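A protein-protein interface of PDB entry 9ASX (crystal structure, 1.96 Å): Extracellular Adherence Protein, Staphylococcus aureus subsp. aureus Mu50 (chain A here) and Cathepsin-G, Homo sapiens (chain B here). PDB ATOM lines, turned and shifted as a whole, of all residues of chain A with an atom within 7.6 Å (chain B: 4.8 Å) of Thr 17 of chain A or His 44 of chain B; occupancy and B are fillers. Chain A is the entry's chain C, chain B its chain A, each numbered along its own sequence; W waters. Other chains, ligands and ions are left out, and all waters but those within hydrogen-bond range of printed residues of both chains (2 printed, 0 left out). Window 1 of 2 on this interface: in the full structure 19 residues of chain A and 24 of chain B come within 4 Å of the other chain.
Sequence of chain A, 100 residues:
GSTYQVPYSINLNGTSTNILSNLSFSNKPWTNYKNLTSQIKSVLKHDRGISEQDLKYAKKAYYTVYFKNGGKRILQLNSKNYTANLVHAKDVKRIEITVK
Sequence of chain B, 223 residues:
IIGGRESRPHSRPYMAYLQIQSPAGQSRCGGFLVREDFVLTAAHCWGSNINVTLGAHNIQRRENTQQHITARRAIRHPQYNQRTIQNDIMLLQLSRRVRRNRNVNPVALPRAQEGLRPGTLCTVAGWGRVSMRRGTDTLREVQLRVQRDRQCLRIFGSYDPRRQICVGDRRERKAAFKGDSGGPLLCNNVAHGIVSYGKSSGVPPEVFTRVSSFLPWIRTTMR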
ATOM      1  N   SER A   9      27.073 -15.954  28.784  1.00  0.00           N
ATOM      2  CA  SER A   9      26.517 -14.653  28.473  1.00  0.00           C
ATOM      3  C   SER A   9      26.595 -14.441  26.970  1.00  0.00           C
ATOM      4  O   SER A   9      27.460 -14.997  26.296  1.00  0.00           O
ATOM      5  CB  SER A   9      27.254 -13.545  29.226  1.00  0.00           C
ATOM      6  OG  SER A   9      28.640 -13.635  28.960  1.00  0.00           O
ATOM      7  N   ILE A  10      25.675 -13.643  26.448  1.00  0.00           N
ATOM      8  CA  ILE A  10      25.671 -13.277  25.035  1.00  0.00           C
ATOM      9  C   ILE A  10      26.030 -11.804  24.904  1.00  0.00           C
ATOM     10  O   ILE A  10      25.406 -10.952  25.541  1.00  0.00           O
ATOM     11  CB  ILE A  10      24.313 -13.566  24.379  1.00  0.00           C
ATOM     12  CG1 ILE A  10      24.017 -15.072  24.432  1.00  0.00           C
ATOM     13  CG2 ILE A  10      24.289 -13.035  22.946  1.00  0.00           C
ATOM     14  CD1 ILE A  10      22.557 -15.427  24.165  1.00  0.00           C
ATOM     15  N   ASN A  11      27.019 -11.507  24.057  1.00  0.00           N
ATOM     16  CA  ASN A  11      27.340 -10.146  23.637  1.00  0.00           C
ATOM     17  C   ASN A  11      26.981 -10.018  22.156  1.00  0.00           C
ATOM     18  O   ASN A  11      27.650 -10.600  21.294  1.00  0.00           O
ATOM     19  CB  ASN A  11      28.813  -9.830  23.901  1.00  0.00           C
ATOM     20  CG  ASN A  11      29.232  -8.476  23.338  1.00  0.00           C
ATOM     21  OD1 ASN A  11      28.398  -7.669  22.919  1.00  0.00           O
ATOM     22  ND2 ASN A  11      30.531  -8.224  23.328  1.00  0.00           N
ATOM     23  N   LEU A  12      25.923  -9.260  21.862  1.00  0.00           N
ATOM     24  CA  LEU A  12      25.426  -9.082  20.498  1.00  0.00           C
ATOM     25  C   LEU A  12      25.531  -7.616  20.098  1.00  0.00           C
ATOM     26  O   LEU A  12      24.954  -6.749  20.764  1.00  0.00           O
ATOM     27  CB  LEU A  12      23.980  -9.561  20.378  1.00  0.00           C
ATOM     28  CG  LEU A  12      23.262  -9.275  19.057  1.00  0.00           C
ATOM     29  CD1 LEU A  12      23.995  -9.909  17.858  1.00  0.00           C
ATOM     30  CD2 LEU A  12      21.825  -9.766  19.133  1.00  0.00           C
ATOM     31  N   THR A  15      25.986  -5.334  22.872  1.00  0.00           N
ATOM     32  CA  THR A  15      24.993  -5.236  23.945  1.00  0.00           C
ATOM     33  C   THR A  15      24.869  -6.575  24.662  1.00  0.00           C
ATOM     34  O   THR A  15      24.950  -7.631  24.029  1.00  0.00           O
ATOM     35  CB  THR A  15      23.609  -4.801  23.414  1.00  0.00           C
ATOM     36  OG1 THR A  15      23.103  -5.768  22.474  1.00  0.00           O
ATOM     37  CG2 THR A  15      23.711  -3.451  22.707  1.00  0.00           C
ATOM     38  N   SER A  16      24.650  -6.521  25.980  1.00  0.00           N
ATOM     39  CA  SER A  16      24.495  -7.708  26.810  1.00  0.00           C
ATOM     40  C   SER A  16      23.461  -7.424  27.890  1.00  0.00           C
ATOM     41  O   SER A  16      23.598  -6.446  28.636  1.00  0.00           O
ATOM     42  CB  SER A  16      25.824  -8.095  27.464  1.00  0.00           C
ATOM     43  OG  SER A  16      25.730  -9.380  28.046  1.00  0.00           O
ATOM     44  N   THR A  17      22.422  -8.256  27.961  1.00  0.00           N
ATOM     45  CA  THR A  17      21.406  -8.081  29.005  1.00  0.00           C
ATOM     46  C   THR A  17      21.987  -8.439  30.378  1.00  0.00           C
ATOM     47  O   THR A  17      23.001  -9.137  30.490  1.00  0.00           O
ATOM     48  CB  THR A  17      20.189  -8.957  28.722  1.00  0.00           C
ATOM     49  OG1 THR A  17      20.614 -10.320  28.592  1.00  0.00           O
ATOM     50  CG2 THR A  17      19.511  -8.543  27.435  1.00  0.00           C
ATOM     51  N   ASN A  18      21.346  -7.934  31.444  1.00  0.00           N
ATOM     52  CA  ASN A  18      21.881  -8.143  32.784  1.00  0.00           C
ATOM     53  C   ASN A  18      21.302  -9.381  33.461  1.00  0.00           C
ATOM     54  O   ASN A  18      21.138  -9.402  34.692  1.00  0.00           O
ATOM     55  CB  ASN A  18      21.668  -6.886  33.636  1.00  0.00           C
ATOM     56  CG  ASN A  18      22.721  -5.833  33.346  1.00  0.00           C
ATOM     57  OD1 ASN A  18      23.925  -6.137  33.326  1.00  0.00           O
ATOM     58  ND2 ASN A  18      22.281  -4.621  33.035  1.00  0.00           N
ATOM     59  N   ILE A  19      20.955 -10.386  32.703  1.00  0.00           N
ATOM     60  CA  ILE A  19      20.418 -11.632  33.241  1.00  0.00           C
ATOM     61  C   ILE A  19      21.583 -12.527  33.640  1.00  0.00           C
ATOM     62  O   ILE A  19      22.683 -12.424  33.075  1.00  0.00           O
ATOM     63  CB  ILE A  19      19.515 -12.313  32.193  1.00  0.00           C
ATOM     64  CG1 ILE A  19      18.739 -13.481  32.815  1.00  0.00           C
ATOM     65  CG2 ILE A  19      20.368 -12.820  31.022  1.00  0.00           C
ATOM     66  CD1 ILE A  19      17.647 -14.028  31.870  1.00  0.00           C
ATOM     67  N   LEU A  20      21.370 -13.398  34.629  1.00  0.00           N
ATOM     68  CA  LEU A  20      22.341 -14.430  34.980  1.00  0.00           C
ATOM     69  C   LEU A  20      21.814 -15.763  34.457  1.00  0.00           C
ATOM     70  O   LEU A  20      20.859 -16.308  35.008  1.00  0.00           O
ATOM     71  CB  LEU A  20      22.568 -14.477  36.489  1.00  0.00           C
ATOM     72  CG  LEU A  20      23.478 -15.586  37.014  1.00  0.00           C
ATOM     73  CD1 LEU A  20      24.856 -15.464  36.397  1.00  0.00           C
ATOM     74  CD2 LEU A  20      23.550 -15.519  38.542  1.00  0.00           C
ATOM     75  N   SER A  21      22.426 -16.278  33.393  1.00  0.00           N
ATOM     76  CA  SER A  21      21.921 -17.452  32.687  1.00  0.00           C
ATOM     77  C   SER A  21      22.917 -18.605  32.713  1.00  0.00           C
ATOM     78  O   SER A  21      24.131 -18.395  32.738  1.00  0.00           O
ATOM     79  CB  SER A  21      21.600 -17.103  31.235  1.00  0.00           C
ATOM     80  OG  SER A  21      20.455 -16.292  31.176  1.00  0.00           O
ATOM     81  N   HIS A  46      17.043 -18.371  21.146  1.00  0.00           N
ATOM     82  CA  HIS A  46      16.003 -18.240  22.161  1.00  0.00           C
ATOM     83  C   HIS A  46      16.133 -16.963  22.991  1.00  0.00           C
ATOM     84  O   HIS A  46      15.111 -16.387  23.389  1.00  0.00           O
ATOM     85  CB  HIS A  46      16.023 -19.466  23.073  1.00  0.00           C
ATOM     86  CG  HIS A  46      14.955 -19.460  24.123  1.00  0.00           C
ATOM     87  ND1 HIS A  46      15.113 -18.836  25.342  1.00  0.00           N
ATOM     88  CD2 HIS A  46      13.715 -20.008  24.138  1.00  0.00           C
ATOM     89  CE1 HIS A  46      14.017 -18.998  26.063  1.00  0.00           C
ATOM     90  NE2 HIS A  46      13.153 -19.704  25.354  1.00  0.00           N
ATOM     91  N   ASP A  47      17.358 -16.508  23.275  1.00  0.00           N
ATOM     92  CA  ASP A  47      17.535 -15.322  24.108  1.00  0.00           C
ATOM     93  C   ASP A  47      17.566 -14.031  23.298  1.00  0.00           C
ATOM     94  O   ASP A  47      17.006 -13.017  23.735  1.00  0.00           O
ATOM     95  CB  ASP A  47      18.822 -15.416  24.930  1.00  0.00           C
ATOM     96  CG  ASP A  47      18.852 -16.619  25.841  1.00  0.00           C
ATOM     97  OD1 ASP A  47      17.841 -17.357  25.898  1.00  0.00           O
ATOM     98  OD2 ASP A  47      19.905 -16.841  26.484  1.00  0.00           O
ATOM     99  N   ARG A  48      18.203 -14.030  22.124  1.00  0.00           N
ATOM    100  CA  ARG A  48      18.331 -12.795  21.367  1.00  0.00           C
ATOM    101  C   ARG A  48      17.801 -12.892  19.942  1.00  0.00           C
ATOM    102  O   ARG A  48      18.084 -11.997  19.143  1.00  0.00           O
ATOM    103  CB  ARG A  48      19.790 -12.326  21.347  1.00  0.00           C
ATOM    104  CG  ARG A  48      20.412 -12.038  22.723  1.00  0.00           C
ATOM    105  CD  ARG A  48      19.695 -10.867  23.457  1.00  0.00           C
ATOM    106  NE  ARG A  48      19.795  -9.625  22.696  1.00  0.00           N
ATOM    107  CZ  ARG A  48      20.841  -8.811  22.723  1.00  0.00           C
ATOM    108  NH1 ARG A  48      21.892  -9.060  23.491  1.00  0.00           N
ATOM    109  NH2 ARG A  48      20.827  -7.711  21.974  1.00  0.00           N
ATOM    110  N   ALA B  42      11.861  -7.467  33.659  1.00  0.00           N
ATOM    111  CA  ALA B  42      12.255  -7.320  32.268  1.00  0.00           C
ATOM    112  C   ALA B  42      11.700  -8.477  31.438  1.00  0.00           C
ATOM    113  O   ALA B  42      11.626  -9.609  31.915  1.00  0.00           O
ATOM    114  CB  ALA B  42      13.782  -7.275  32.157  1.00  0.00           C
ATOM    115  N   ALA B  43      11.334  -8.195  30.178  1.00  0.00           N
ATOM    116  CA  ALA B  43      10.819  -9.272  29.320  1.00  0.00           C
ATOM    117  C   ALA B  43      11.892 -10.312  28.955  1.00  0.00           C
ATOM    118  O   ALA B  43      11.554 -11.480  28.735  1.00  0.00           O
ATOM    119  CB  ALA B  43      10.197  -8.675  28.046  1.00  0.00           C
ATOM    120  N   HIS B  44      13.181  -9.939  28.910  1.00  0.00           N
ATOM    121  CA  HIS B  44      14.188 -10.966  28.642  1.00  0.00           C
ATOM    122  C   HIS B  44      14.388 -11.942  29.815  1.00  0.00           C
ATOM    123  O   HIS B  44      15.183 -12.876  29.670  1.00  0.00           O
ATOM    124  CB  HIS B  44      15.535 -10.333  28.228  1.00  0.00           C
ATOM    125  CG  HIS B  44      16.275  -9.668  29.347  1.00  0.00           C
ATOM    126  ND1 HIS B  44      16.234  -8.304  29.563  1.00  0.00           N
ATOM    127  CD2 HIS B  44      17.081 -10.180  30.310  1.00  0.00           C
ATOM    128  CE1 HIS B  44      16.978  -8.007  30.616  1.00  0.00           C
ATOM    129  NE2 HIS B  44      17.510  -9.125  31.083  1.00  0.00           N
ATOM    130  N   CYS B  45      13.701 -11.756  30.953  1.00  0.00           N
ATOM    131  CA  CYS B  45      13.667 -12.728  32.047  1.00  0.00           C
ATOM    132  C   CYS B  45      12.545 -13.766  31.908  1.00  0.00           C
ATOM    133  O   CYS B  45      12.301 -14.537  32.851  1.00  0.00           O
ATOM    134  CB  CYS B  45      13.521 -12.004  33.400  1.00  0.00           C
ATOM    135  SG  CYS B  45      14.909 -10.882  33.738  1.00  0.00           S
ATOM    136  N   TRP B  46      11.842 -13.786  30.784  1.00  0.00           N
ATOM    137  CA  TRP B  46      10.756 -14.739  30.596  1.00  0.00           C
ATOM    138  C   TRP B  46      11.288 -16.174  30.496  1.00  0.00           C
ATOM    139  O   TRP B  46      12.400 -16.422  30.031  1.00  0.00           O
ATOM    140  CB  TRP B  46       9.951 -14.367  29.342  1.00  0.00           C
ATOM    141  CG  TRP B  46       8.762 -15.263  29.067  1.00  0.00           C
ATOM    142  CD1 TRP B  46       7.458 -15.038  29.401  1.00  0.00           C
ATOM    143  CD2 TRP B  46       8.788 -16.511  28.382  1.00  0.00           C
ATOM    144  NE1 TRP B  46       6.667 -16.078  28.970  1.00  0.00           N
ATOM    145  CE2 TRP B  46       7.463 -16.995  28.338  1.00  0.00           C
ATOM    146  CE3 TRP B  46       9.808 -17.269  27.796  1.00  0.00           C
ATOM    147  CZ2 TRP B  46       7.136 -18.215  27.754  1.00  0.00           C
ATOM    148  CZ3 TRP B  46       9.483 -18.476  27.213  1.00  0.00           C
ATOM    149  CH2 TRP B  46       8.154 -18.932  27.187  1.00  0.00           C
ATOM    150  N   TYR B  80       7.772  -6.612  22.525  1.00  0.00           N
ATOM    151  CA  TYR B  80       9.125  -6.937  22.974  1.00  0.00           C
ATOM    152  C   TYR B  80       9.963  -7.490  21.825  1.00  0.00           C
ATOM    153  O   TYR B  80       9.531  -8.398  21.106  1.00  0.00           O
ATOM    154  CB  TYR B  80       9.067  -7.969  24.102  1.00  0.00           C
ATOM    155  CG  TYR B  80      10.410  -8.547  24.431  1.00  0.00           C
ATOM    156  CD1 TYR B  80      11.472  -7.724  24.763  1.00  0.00           C
ATOM    157  CD2 TYR B  80      10.624  -9.925  24.402  1.00  0.00           C
ATOM    158  CE1 TYR B  80      12.716  -8.242  25.057  1.00  0.00           C
ATOM    159  CE2 TYR B  80      11.868 -10.455  24.728  1.00  0.00           C
ATOM    160  CZ  TYR B  80      12.907  -9.604  25.041  1.00  0.00           C
ATOM    161  OH  TYR B  80      14.147 -10.103  25.349  1.00  0.00           O
ATOM    162  N   ILE B  85      16.363  -5.556  22.110  1.00  0.00           N
ATOM    163  CA  ILE B  85      16.055  -5.418  23.538  1.00  0.00           C
ATOM    164  C   ILE B  85      15.155  -4.200  23.721  1.00  0.00           C
ATOM    165  O   ILE B  85      15.365  -3.396  24.633  1.00  0.00           O
ATOM    166  CB  ILE B  85      17.320  -5.314  24.418  1.00  0.00           C
ATOM    167  CG1 ILE B  85      18.394  -6.307  23.983  1.00  0.00           C
ATOM    168  CG2 ILE B  85      16.977  -5.586  25.915  1.00  0.00           C
ATOM    169  CD1 ILE B  85      19.774  -6.000  24.593  1.00  0.00           C
ATOM    170  N   ASP B  88      11.343  -3.862  26.601  1.00  0.00           N
ATOM    171  CA  ASP B  88      11.814  -4.909  27.506  1.00  0.00           C
ATOM    172  C   ASP B  88      11.118  -4.770  28.863  1.00  0.00           C
ATOM    173  O   ASP B  88      11.673  -4.270  29.841  1.00  0.00           O
ATOM    174  CB  ASP B  88      13.330  -4.814  27.663  1.00  0.00           C
ATOM    175  CG  ASP B  88      13.921  -6.001  28.426  1.00  0.00           C
ATOM    176  OD1 ASP B  88      13.243  -7.047  28.507  1.00  0.00           O
ATOM    177  OD2 ASP B  88      15.078  -5.902  28.927  1.00  0.00           O
ATOM    178  N   LYS B 178      25.230  -8.827  36.164  1.00  0.00           N
ATOM    179  CA  LYS B 178      24.558 -10.060  35.747  1.00  0.00           C
ATOM    180  C   LYS B 178      23.706 -10.623  36.880  1.00  0.00           C
ATOM    181  O   LYS B 178      24.228 -10.988  37.941  1.00  0.00           O
ATOM    182  CB  LYS B 178      25.570 -11.110  35.291  1.00  0.00           C
ATOM    183  CG  LYS B 178      26.393 -10.725  34.051  1.00  0.00           C
ATOM    184  CD  LYS B 178      25.504 -10.096  32.976  1.00  0.00           C
ATOM    185  CE  LYS B 178      25.966 -10.447  31.548  1.00  0.00           C
ATOM    186  NZ  LYS B 178      27.080  -9.603  31.094  1.00  0.00           N
ATOM    187  N   SER B 181      19.056  -7.847  36.228  1.00  0.00           N
ATOM    188  CA  SER B 181      17.990  -7.539  35.281  1.00  0.00           C
ATOM    189  C   SER B 181      16.621  -7.581  35.956  1.00  0.00           C
ATOM    190  O   SER B 181      16.347  -8.455  36.777  1.00  0.00           O
ATOM    191  CB  SER B 181      17.998  -8.543  34.133  1.00  0.00           C
ATOM    192  OG  SER B 181      18.850  -8.107  33.111  1.00  0.00           O
ATOM    193  N   VAL B 195      16.089  -2.493  35.287  1.00  0.00           N
ATOM    194  CA  VAL B 195      17.404  -2.889  34.778  1.00  0.00           C
ATOM    195  C   VAL B 195      17.246  -3.709  33.502  1.00  0.00           C
ATOM    196  O   VAL B 195      16.528  -4.713  33.484  1.00  0.00           O
ATOM    197  CB  VAL B 195      18.172  -3.710  35.825  1.00  0.00           C
ATOM    198  CG1 VAL B 195      19.543  -4.165  35.252  1.00  0.00           C
ATOM    199  CG2 VAL B 195      18.335  -2.953  37.146  1.00  0.00           C
ATOM    200  N   SER B 196      17.946  -3.314  32.434  1.00  0.00           N
ATOM    201  CA  SER B 196      17.753  -4.048  31.189  1.00  0.00           C
ATOM    202  C   SER B 196      19.063  -4.549  30.578  1.00  0.00           C
ATOM    203  O   SER B 196      19.323  -5.764  30.577  1.00  0.00           O
ATOM    204  CB  SER B 196      16.959  -3.183  30.191  1.00  0.00           C
ATOM    205  OG  SER B 196      16.711  -3.880  28.964  1.00  0.00           O
ATOM    206  N   TYR B 197      19.897  -3.655  30.050  1.00  0.00           N
ATOM    207  CA  TYR B 197      21.137  -4.128  29.440  1.00  0.00           C
ATOM    208  C   TYR B 197      22.234  -3.070  29.500  1.00  0.00           C
ATOM    209  O   TYR B 197      22.000  -1.913  29.850  1.00  0.00           O
ATOM    210  CB  TYR B 197      20.912  -4.551  27.977  1.00  0.00           C
ATOM    211  CG  TYR B 197      20.597  -3.417  26.988  1.00  0.00           C
ATOM    212  CD1 TYR B 197      21.610  -2.774  26.270  1.00  0.00           C
ATOM    213  CD2 TYR B 197      19.299  -3.035  26.738  1.00  0.00           C
ATOM    214  CE1 TYR B 197      21.320  -1.757  25.337  1.00  0.00           C
ATOM    215  CE2 TYR B 197      18.996  -2.015  25.809  1.00  0.00           C
ATOM    216  CZ  TYR B 197      20.013  -1.398  25.104  1.00  0.00           C
ATOM    217  OH  TYR B 197      19.695  -0.408  24.182  1.00  0.00           O
HETATM  218  O   HOH W   1      20.866  -1.887  32.792  1.00  0.00           O
HETATM  219  O   HOH W   2      14.668 -12.640  25.233  1.00  0.00           O
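Of chain A, only Thr 17 (3.6 Å) and Ile 19 (3.5 Å) come within 4 Å of His 44 of chain B.
No residue of chain A comes within 4 Å of Ala 43 of chain B.
Of the printed residues of chain A, Lys 178 of chain B touches Ser 16 (3.3 Å), Thr 17 (3.4 Å), Asn 18 (3.6 Å) and Ile 19 (3.7 Å).
Of the printed residues of chain B, Ile 19 of chain A touches His 44 (3.5 Å), Lys 178 (3.7 Å) and Ser 181 (3.1 Å).
Printed residues of chain B within 4 Å of Thr 15 of chain A: Ile 85 and Tyr 197.
Printed residues of chain B within 4 Å of Ser 16 of chain A: Lys 178 and Tyr 197.
The nearest residue of chain B that does not touch Thr 17 of chain A is Ser 181 of chain B (4.2 Å).
The nearest residue of chain A that does not touch His 44 of chain B is Asn 18 of chain A (4.03 Å).
The nearest printed residue of chain A that does not touch Ile 85 of chain B is Ser 16 of chain A (5.1 Å).
Water W2 lies within hydrogen-bond range of OH of Tyr 80 of chain B and O of Asp 47 of chain A.
Water W1 lies within hydrogen-bond range of the side-chain amide nitrogen (ND2) of Asn 18 of chain A (3.1 Å), the backbone carbonyl oxygen (O) of Tyr 197 of chain B (3.2 Å) and the backbone NH (N) of Ser 196 of chain B (3.3 Å).
Printed residues of chain B that touch a printed residue of chain A: His 44, Ile 85, Lys 178, Ser 181, Val 195, Ser 196 and Tyr 197.
Hydrophobic or aromatic side chains of chain A that line the printed part of chain B: Ile 19.
Among the printed residues, 18 pairs touch across the chains.
Among the printed residues, no Asp or Glu carboxylate lies within 4 Å of a Lys or Arg side-chain nitrogen of the other chain.
Among the printed residues, pairs that only touch across the chains: Thr 15 of chain A with Ile 85 of chain B (3.95 Å), Thr 15 of chain A with Tyr 197 of chain B (3.9 Å), Ser 16 of chain A with Tyr 197 of chain B (3.4 Å), Thr 17 of chain A with His 44 of chain B (3.6 Å), Thr 17 of chain A with Ile 85 of chain B (3.8 Å), Thr 17 of chain A with Lys 178 of chain B (3.4 Å), Thr 17 of chain A with Ser 196 of chain B (3.5 Å), Thr 17 of chain A with Tyr 197 of chain B (3.7 Å), Asn 18 of chain A with Lys 178 of chain B (3.6 Å), Asn 18 of chain A with Val 195 of chain B (3.6 Å), Asn 18 of chain A with Tyr 197 of chain B (3.8 Å), Ile 19 of chain A with His 44 of chain B (3.5 Å), Ile 19 of chain A with Lys 178 of chain B (3.7 Å) and Arg 48 of chain A with Ile 85 of chain B (3.3 Å).
The side-chain amino group (NZ) of Lys 178 of chain B sits at hydrogen-bond distance from the side-chain hydroxyl (OG) of Ser 16 of chain A.
The side-chain hydroxyl of Ser 181 of chain B lies close to the backbone NH of Asn 18 of chain A, 3.0 Å away.
The side-chain hydroxyl (OG) of Ser 181 of chain B is in hydrogen-bond range of the backbone NH (N) of Ile 19 of chain A.
The backbone carbonyl oxygen (O) of Ser 196 of chain B is in hydrogen-bond range of the backbone NH (N) of Asn 18 of chain A.
OD2 of Asp 88 of chain B sits at hydrogen-bond distance from ND1 of His 44 of chain B.
A ring nitrogen (NE2) of His 44 of chain B sits at hydrogen-bond distance from the side-chain hydroxyl (OG) of Ser 181 of chain B, at 2.6 Å.
O of Ser 196 of chain B is in hydrogen-bond range of OG of Ser 181 of chain B, 3.5 Å away.
The backbone carbonyl oxygen (O) of Ile 10 of chain A lies within hydrogen-bond range of the side-chain hydroxyl (OG) of Ser 16 of chain A (3.0 Å).
The backbone NH (N) of Thr 15 of chain A lies within hydrogen-bond range of the side-chain amide oxygen (OD1) of Asn 11 of chain A (3.4 Å).
The backbone carbonyl oxygen (O) of Leu 12 of chain A lies within hydrogen-bond range of the side-chain hydroxyl (OG1) of Thr 15 of chain A (2.7 Å).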
